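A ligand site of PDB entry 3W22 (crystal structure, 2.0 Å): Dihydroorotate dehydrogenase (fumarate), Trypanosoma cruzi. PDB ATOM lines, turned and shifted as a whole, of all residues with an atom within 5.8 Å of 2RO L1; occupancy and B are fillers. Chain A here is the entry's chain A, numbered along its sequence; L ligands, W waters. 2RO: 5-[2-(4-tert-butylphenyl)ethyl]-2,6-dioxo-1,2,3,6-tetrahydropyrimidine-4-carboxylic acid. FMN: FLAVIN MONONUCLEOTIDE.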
ATOM      1  N   LYS A  44     -30.336  12.320   1.816  1.00  0.00           N
ATOM      2  CA  LYS A  44     -29.077  11.666   2.112  1.00  0.00           C
ATOM      3  C   LYS A  44     -29.270  10.348   2.865  1.00  0.00           C
ATOM      4  O   LYS A  44     -30.046  10.318   3.812  1.00  0.00           O
ATOM      5  CB  LYS A  44     -28.279  12.563   2.999  1.00  0.00           C
ATOM      6  CG  LYS A  44     -27.022  11.950   3.562  1.00  0.00           C
ATOM      7  CD  LYS A  44     -25.973  11.579   2.557  1.00  0.00           C
ATOM      8  CE  LYS A  44     -24.794  10.865   3.228  1.00  0.00           C
ATOM      9  NZ  LYS A  44     -23.664  10.509   2.269  1.00  0.00           N
ATOM     10  N   SER A  45     -28.463   9.348   2.539  1.00  0.00           N
ATOM     11  CA  SER A  45     -28.582   8.019   3.133  1.00  0.00           C
ATOM     12  C   SER A  45     -28.326   8.207   4.609  1.00  0.00           C
ATOM     13  O   SER A  45     -27.351   8.799   4.982  1.00  0.00           O
ATOM     14  CB  SER A  45     -27.553   7.052   2.580  1.00  0.00           C
ATOM     15  OG  SER A  45     -27.906   6.481   1.343  1.00  0.00           O
ATOM     16  N   ARG A  51     -24.344  11.258  12.194  1.00  0.00           N
ATOM     17  CA  ARG A  51     -22.916  11.030  12.003  1.00  0.00           C
ATOM     18  C   ARG A  51     -22.197  12.245  11.424  1.00  0.00           C
ATOM     19  O   ARG A  51     -22.723  12.889  10.519  1.00  0.00           O
ATOM     20  CB  ARG A  51     -22.694   9.888  11.012  1.00  0.00           C
ATOM     21  CG  ARG A  51     -23.089   8.512  11.496  1.00  0.00           C
ATOM     22  CD  ARG A  51     -22.990   7.492  10.406  1.00  0.00           C
ATOM     23  NE  ARG A  51     -21.660   7.424   9.767  1.00  0.00           N
ATOM     24  CZ  ARG A  51     -20.683   6.650  10.205  1.00  0.00           C
ATOM     25  NH1 ARG A  51     -20.818   5.920  11.296  1.00  0.00           N
ATOM     26  NH2 ARG A  51     -19.558   6.633   9.582  1.00  0.00           N
ATOM     27  N   ASN A  54     -16.436  11.166   7.767  1.00  0.00           N
ATOM     28  CA  ASN A  54     -14.983  11.149   7.684  1.00  0.00           C
ATOM     29  C   ASN A  54     -14.337  12.560   7.758  1.00  0.00           C
ATOM     30  O   ASN A  54     -14.990  13.610   7.492  1.00  0.00           O
ATOM     31  CB  ASN A  54     -14.567  10.427   6.382  1.00  0.00           C
ATOM     32  CG  ASN A  54     -14.661   8.954   6.479  1.00  0.00           C
ATOM     33  OD1 ASN A  54     -14.691   8.414   7.581  1.00  0.00           O
ATOM     34  ND2 ASN A  54     -14.678   8.279   5.367  1.00  0.00           N
ATOM     35  N   ASN A  68     -14.964  10.442  -3.646  1.00  0.00           N
ATOM     36  CA  ASN A  68     -15.435  10.742  -2.339  1.00  0.00           C
ATOM     37  C   ASN A  68     -15.272   9.565  -1.396  1.00  0.00           C
ATOM     38  O   ASN A  68     -15.505   8.398  -1.748  1.00  0.00           O
ATOM     39  CB  ASN A  68     -16.908  11.219  -2.314  1.00  0.00           C
ATOM     40  CG  ASN A  68     -17.908  10.069  -2.211  1.00  0.00           C
ATOM     41  OD1 ASN A  68     -18.191   9.528  -1.095  1.00  0.00           O
ATOM     42  ND2 ASN A  68     -18.452   9.679  -3.347  1.00  0.00           N
ATOM     43  N   SER A  69     -14.967   9.916  -0.168  1.00  0.00           N
ATOM     44  CA  SER A  69     -15.139   8.987   0.913  1.00  0.00           C
ATOM     45  C   SER A  69     -15.760   9.733   2.084  1.00  0.00           C
ATOM     46  O   SER A  69     -15.128  10.001   3.114  1.00  0.00           O
ATOM     47  CB  SER A  69     -13.805   8.285   1.165  1.00  0.00           C
ATOM     48  OG  SER A  69     -13.968   7.599   2.382  1.00  0.00           O
ATOM     49  N   MET A  70     -17.046  10.046   1.918  1.00  0.00           N
ATOM     50  CA  MET A  70     -17.712  10.940   2.854  1.00  0.00           C
ATOM     51  C   MET A  70     -17.870  10.256   4.255  1.00  0.00           C
ATOM     52  O   MET A  70     -17.795  10.890   5.272  1.00  0.00           O
ATOM     53  CB  MET A  70     -19.065  11.366   2.347  1.00  0.00           C
ATOM     54  CG  MET A  70     -19.160  11.974   0.991  1.00  0.00           C
ATOM     55  SD  MET A  70     -18.251  13.500   0.870  1.00  0.00           S
ATOM     56  CE  MET A  70     -19.231  14.617   1.808  1.00  0.00           C
ATOM     57  N   GLY A  71     -18.071   8.952   4.294  1.00  0.00           N
ATOM     58  CA  GLY A  71     -18.317   8.267   5.573  1.00  0.00           C
ATOM     59  C   GLY A  71     -19.723   8.430   6.136  1.00  0.00           C
ATOM     60  O   GLY A  71     -19.868   8.509   7.348  1.00  0.00           O
ATOM     61  N   LEU A  72     -20.720   8.574   5.279  1.00  0.00           N
ATOM     62  CA  LEU A  72     -22.131   8.669   5.685  1.00  0.00           C
ATOM     63  C   LEU A  72     -22.369   9.772   6.723  1.00  0.00           C
ATOM     64  O   LEU A  72     -23.009   9.568   7.729  1.00  0.00           O
ATOM     65  CB  LEU A  72     -22.579   7.287   6.245  1.00  0.00           C
ATOM     66  CG  LEU A  72     -23.928   6.653   6.064  1.00  0.00           C
ATOM     67  CD1 LEU A  72     -24.553   6.915   4.704  1.00  0.00           C
ATOM     68  CD2 LEU A  72     -23.781   5.139   6.371  1.00  0.00           C
ATOM     69  N   PRO A  73     -21.884  10.966   6.468  1.00  0.00           N
ATOM     70  CA  PRO A  73     -22.358  12.068   7.309  1.00  0.00           C
ATOM     71  C   PRO A  73     -23.862  12.330   7.101  1.00  0.00           C
ATOM     72  O   PRO A  73     -24.328  12.381   5.959  1.00  0.00           O
ATOM     73  CB  PRO A  73     -21.546  13.250   6.837  1.00  0.00           C
ATOM     74  CG  PRO A  73     -21.327  12.996   5.387  1.00  0.00           C
ATOM     75  CD  PRO A  73     -21.130  11.467   5.283  1.00  0.00           C
ATOM     76  N   SER A 100     -29.307   3.712   5.013  1.00  0.00           N
ATOM     77  CA  SER A 100     -28.089   2.963   4.880  1.00  0.00           C
ATOM     78  C   SER A 100     -27.580   2.586   6.233  1.00  0.00           C
ATOM     79  O   SER A 100     -26.470   2.991   6.661  1.00  0.00           O
ATOM     80  CB  SER A 100     -27.057   3.837   4.137  1.00  0.00           C
ATOM     81  OG  SER A 100     -25.832   3.162   4.111  1.00  0.00           O
ATOM     82  N   ASN A 128     -30.064   1.514   0.515  1.00  0.00           N
ATOM     83  CA  ASN A 128     -28.718   1.585  -0.042  1.00  0.00           C
ATOM     84  C   ASN A 128     -28.019   0.289   0.295  1.00  0.00           C
ATOM     85  O   ASN A 128     -27.635   0.069   1.447  1.00  0.00           O
ATOM     86  CB  ASN A 128     -27.949   2.744   0.589  1.00  0.00           C
ATOM     87  CG  ASN A 128     -26.611   2.971  -0.024  1.00  0.00           C
ATOM     88  OD1 ASN A 128     -26.157   2.192  -0.797  1.00  0.00           O
ATOM     89  ND2 ASN A 128     -25.973   4.077   0.344  1.00  0.00           N
ATOM     90  N   SER A 130     -25.035  -0.521  -0.894  1.00  0.00           N
ATOM     91  CA  SER A 130     -23.628  -0.335  -0.526  1.00  0.00           C
ATOM     92  C   SER A 130     -23.472  -0.060   0.974  1.00  0.00           C
ATOM     93  O   SER A 130     -22.384   0.182   1.417  1.00  0.00           O
ATOM     94  CB  SER A 130     -22.972   0.738  -1.321  1.00  0.00           C
ATOM     95  OG  SER A 130     -22.956   0.345  -2.680  1.00  0.00           O
ATOM     96  N   CYS A 131     -24.525  -0.144   1.780  1.00  0.00           N
ATOM     97  CA  CYS A 131     -24.314  -0.007   3.218  1.00  0.00           C
ATOM     98  C   CYS A 131     -23.168  -0.960   3.613  1.00  0.00           C
ATOM     99  O   CYS A 131     -23.025  -2.070   3.036  1.00  0.00           O
ATOM    100  CB  CYS A 131     -25.599  -0.256   4.004  1.00  0.00           C
ATOM    101  SG  CYS A 131     -26.397  -1.862   3.761  1.00  0.00           S
ATOM    102  N   PRO A 132     -22.286  -0.498   4.518  1.00  0.00           N
ATOM    103  CA  PRO A 132     -21.085  -1.284   4.813  1.00  0.00           C
ATOM    104  C   PRO A 132     -21.443  -2.551   5.613  1.00  0.00           C
ATOM    105  O   PRO A 132     -22.369  -2.518   6.391  1.00  0.00           O
ATOM    106  CB  PRO A 132     -20.203  -0.311   5.593  1.00  0.00           C
ATOM    107  CG  PRO A 132     -21.176   0.636   6.224  1.00  0.00           C
ATOM    108  CD  PRO A 132     -22.310   0.786   5.242  1.00  0.00           C
ATOM    109  N   ASN A 195     -24.495   3.164  -7.811  1.00  0.00           N
ATOM    110  CA  ASN A 195     -23.731   3.885  -6.854  1.00  0.00           C
ATOM    111  C   ASN A 195     -22.306   4.165  -7.434  1.00  0.00           C
ATOM    112  O   ASN A 195     -21.982   3.782  -8.581  1.00  0.00           O
ATOM    113  CB  ASN A 195     -23.598   3.095  -5.521  1.00  0.00           C
ATOM    114  CG  ASN A 195     -23.512   4.011  -4.321  1.00  0.00           C
ATOM    115  OD1 ASN A 195     -22.634   4.880  -4.256  1.00  0.00           O
ATOM    116  ND2 ASN A 195     -24.400   3.825  -3.348  1.00  0.00           N
ATOM    117  N   SER A 196     -21.479   4.869  -6.667  1.00  0.00           N
ATOM    118  CA  SER A 196     -20.087   5.163  -7.114  1.00  0.00           C
ATOM    119  C   SER A 196     -19.243   3.905  -7.430  1.00  0.00           C
ATOM    120  O   SER A 196     -19.516   2.771  -6.942  1.00  0.00           O
ATOM    121  CB  SER A 196     -19.394   6.120  -6.129  1.00  0.00           C
ATOM    122  OG  SER A 196     -19.339   5.571  -4.863  1.00  0.00           O
ATOM    123  N   LYS A 215      -8.968   6.774   4.114  1.00  0.00           N
ATOM    124  CA  LYS A 215      -8.651   5.556   3.337  1.00  0.00           C
ATOM    125  C   LYS A 215      -7.446   5.707   2.403  1.00  0.00           C
ATOM    126  O   LYS A 215      -7.419   5.147   1.339  1.00  0.00           O
ATOM    127  CB  LYS A 215      -9.909   5.101   2.528  1.00  0.00           C
ATOM    128  CG  LYS A 215     -11.156   4.768   3.360  1.00  0.00           C
ATOM    129  CD  LYS A 215     -12.388   4.417   2.478  1.00  0.00           C
ATOM    130  CE  LYS A 215     -12.065   3.412   1.368  1.00  0.00           C
ATOM    131  NZ  LYS A 215     -13.182   2.609   0.777  1.00  0.00           N
ATOM    132  N   GLY A 220     -14.893   6.478  -3.764  1.00  0.00           N
ATOM    133  CA  GLY A 220     -15.769   6.181  -4.846  1.00  0.00           C
ATOM    134  C   GLY A 220     -15.777   7.204  -5.950  1.00  0.00           C
ATOM    135  O   GLY A 220     -15.727   8.416  -5.708  1.00  0.00           O
HETATM  136  OAD 2RO L   1     -21.302   8.554   2.516  1.00  0.00           O
HETATM  137  CAP 2RO L   1     -20.607   8.051   1.617  1.00  0.00           C
HETATM  138  OAG 2RO L   1     -19.356   8.068   1.698  1.00  0.00           O
HETATM  139  CAS 2RO L   1     -21.171   7.422   0.447  1.00  0.00           C
HETATM  140  NAN 2RO L   1     -20.538   7.765  -0.779  1.00  0.00           N
HETATM  141  CAU 2RO L   1     -20.941   7.202  -1.995  1.00  0.00           C
HETATM  142  OAE 2RO L   1     -20.417   7.506  -3.077  1.00  0.00           O
HETATM  143  NAO 2RO L   1     -21.952   6.258  -1.964  1.00  0.00           N
HETATM  144  CAV 2RO L   1     -22.539   5.808  -0.748  1.00  0.00           C
HETATM  145  OAF 2RO L   1     -23.402   4.894  -0.846  1.00  0.00           O
HETATM  146  CAT 2RO L   1     -22.133   6.395   0.489  1.00  0.00           C
HETATM  147  CAM 2RO L   1     -22.668   6.034   1.709  1.00  0.00           C
HETATM  148  CAL 2RO L   1     -22.419   4.511   1.946  1.00  0.00           C
HETATM  149  CAQ 2RO L   1     -21.089   4.460   2.490  1.00  0.00           C
HETATM  150  CAH 2RO L   1     -20.002   4.415   1.631  1.00  0.00           C
HETATM  151  CAJ 2RO L   1     -18.686   4.388   2.092  1.00  0.00           C
HETATM  152  CAR 2RO L   1     -18.369   4.409   3.477  1.00  0.00           C
HETATM  153  CAW 2RO L   1     -16.934   4.422   3.817  1.00  0.00           C
HETATM  154  CAB 2RO L   1     -16.110   3.307   3.083  1.00  0.00           C
HETATM  155  CAC 2RO L   1     -16.317   5.801   3.333  1.00  0.00           C
HETATM  156  CAA 2RO L   1     -16.668   4.310   5.363  1.00  0.00           C
HETATM  157  CAK 2RO L   1     -19.471   4.488   4.330  1.00  0.00           C
HETATM  158  CAI 2RO L   1     -20.796   4.514   3.846  1.00  0.00           C
HETATM  159  N1  FMN L   2     -25.090   7.164  -2.814  1.00  0.00           N
HETATM  160  C2  FMN L   2     -25.947   6.748  -1.848  1.00  0.00           C
HETATM  161  O2  FMN L   2     -26.709   5.794  -2.148  1.00  0.00           O
HETATM  162  N3  FMN L   2     -25.991   7.288  -0.643  1.00  0.00           N
HETATM  163  C4  FMN L   2     -25.298   8.347  -0.262  1.00  0.00           C
HETATM  164  O4  FMN L   2     -25.421   8.879   0.870  1.00  0.00           O
HETATM  165  C4A FMN L   2     -24.363   8.893  -1.227  1.00  0.00           C
HETATM  166  N5  FMN L   2     -23.581   9.920  -0.936  1.00  0.00           N
HETATM  167  C5A FMN L   2     -22.782  10.514  -1.875  1.00  0.00           C
HETATM  168  C6  FMN L   2     -22.050  11.706  -1.574  1.00  0.00           C
HETATM  169  C7  FMN L   2     -21.212  12.273  -2.569  1.00  0.00           C
HETATM  170  C7M FMN L   2     -20.444  13.519  -2.207  1.00  0.00           C
HETATM  171  C8  FMN L   2     -21.189  11.698  -3.937  1.00  0.00           C
HETATM  172  C8M FMN L   2     -20.320  12.242  -5.060  1.00  0.00           C
HETATM  173  C9  FMN L   2     -21.907  10.546  -4.205  1.00  0.00           C
HETATM  174  C9A FMN L   2     -22.719   9.938  -3.234  1.00  0.00           C
HETATM  175  N10 FMN L   2     -23.488   8.774  -3.515  1.00  0.00           N
HETATM  176  C10 FMN L   2     -24.320   8.251  -2.545  1.00  0.00           C
HETATM  177  C1' FMN L   2     -23.484   8.142  -4.827  1.00  0.00           C
HETATM  178  C2' FMN L   2     -24.310   8.963  -5.763  1.00  0.00           C
HETATM  179  O2' FMN L   2     -25.650   8.752  -5.343  1.00  0.00           O
HETATM  180  C3' FMN L   2     -24.156   8.378  -7.155  1.00  0.00           C
HETATM  181  O3' FMN L   2     -24.646   7.040  -7.047  1.00  0.00           O
HETATM  182  C4' FMN L   2     -22.712   8.421  -7.736  1.00  0.00           C
HETATM  183  O4' FMN L   2     -22.055   9.670  -7.359  1.00  0.00           O
HETATM  184  C5' FMN L   2     -22.698   8.351  -9.282  1.00  0.00           C
HETATM  185  O5' FMN L   2     -23.480   9.340  -9.923  1.00  0.00           O
HETATM  186  P   FMN L   2     -22.733  10.570 -10.687  1.00  0.00           P
HETATM  187  O1P FMN L   2     -23.850  11.500 -11.174  1.00  0.00           O
HETATM  188  O2P FMN L   2     -21.775   9.916 -11.580  1.00  0.00           O
HETATM  189  O3P FMN L   2     -21.939  11.106  -9.520  1.00  0.00           O
HETATM  190  O   HOH W   1     -17.680   6.628  -0.012  1.00  0.00           O
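OD1 of Asn 68 sits at hydrogen-bond distance from N of Met 70, at 3.3 Å.
The backbone carbonyl oxygen of Asn 68 is in hydrogen-bond range of the backbone NH of Gly 220.
OD1 of Asn 128 is in hydrogen-bond range of N of Ser 130, at 2.9 Å.
O of Asn 128 sits at hydrogen-bond distance from SG of Cys 131, 3.3 Å away.
The side-chain hydroxyl of Ser 45 sits at hydrogen-bond distance from the side-chain amide nitrogen of Asn 128.
The guanidinium group of Arg 51 sits at hydrogen-bond distance from the backbone carbonyl oxygen of Gly 71 (2.9 Å).
O of Met 70 sits at hydrogen-bond distance from N of Asn 54, 2.9 Å away.
The backbone carbonyl oxygen (O) of Ser 69 sits at hydrogen-bond distance from the side-chain amide nitrogen (ND2) of Asn 54, 2.9 Å away.
Merely in contact with 2RO L1: Asn 54, Ser 69 and Lys 215.
Hydrophobic or aromatic side chains within 4 Å of 2RO L1: Met 70 and Leu 72.
Within 4 Å of 2RO L1: Lys 44, Asn 54, Asn 68, Ser 69, Met 70, Gly 71, Leu 72, Asn 128, Asn 195, Ser 196 and Lys 215.
The nearest printed residue that does not touch 2RO L1 is Pro 73 (4.02 Å).
The side-chain amide oxygen of Asn 195 is in hydrogen-bond range of a nitrogen (NAO) of 2RO L1, at 2.8 Å.
An oxygen (OAD) of 2RO L1 is in hydrogen-bond range of the backbone NH of Leu 72, at 2.8 Å.
The side-chain hydroxyl (OG) of Ser 196 sits at hydrogen-bond distance from an oxygen (OAE) of 2RO L1.
An oxygen (OAE) of 2RO L1 is in hydrogen-bond range of the side-chain amide nitrogen (ND2) of Asn 68.
The side-chain amide nitrogen (ND2) of Asn 128 is in hydrogen-bond range of an oxygen (OAF) of 2RO L1, at 2.9 Å.
N of Gly 71 lies within hydrogen-bond range of OAG of 2RO L1.
N of Met 70 sits at hydrogen-bond distance from OAG of 2RO L1 (3.0 Å).
The side-chain amino group (NZ) of Lys 44 lies within salt-bridge range of an oxygen (OAD) of 2RO L1, 3.1 Å away.
An oxygen (O2) of FMN L2 lies within hydrogen-bond range of the side-chain amide nitrogen (ND2) of Asn 195, 3.3 Å away.
ND2 of Asn 128 sits at hydrogen-bond distance from O2 of FMN L2 (3.1 Å).
An oxygen (O4) of FMN L2 lies within hydrogen-bond range of the side-chain amino group (NZ) of Lys 44.
The side-chain hydroxyl of Ser 45 is in hydrogen-bond range of a nitrogen (N3) of FMN L2.
A nitrogen (N1) of FMN L2 sits close to a nitrogen (NAO) of 2RO L1 (3.4 Å).
Water W1 lies within hydrogen-bond range of an oxygen (OAG) of 2RO L1 (2.8 Å) and the side-chain amide oxygen of Asn 68 (3.1 Å).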
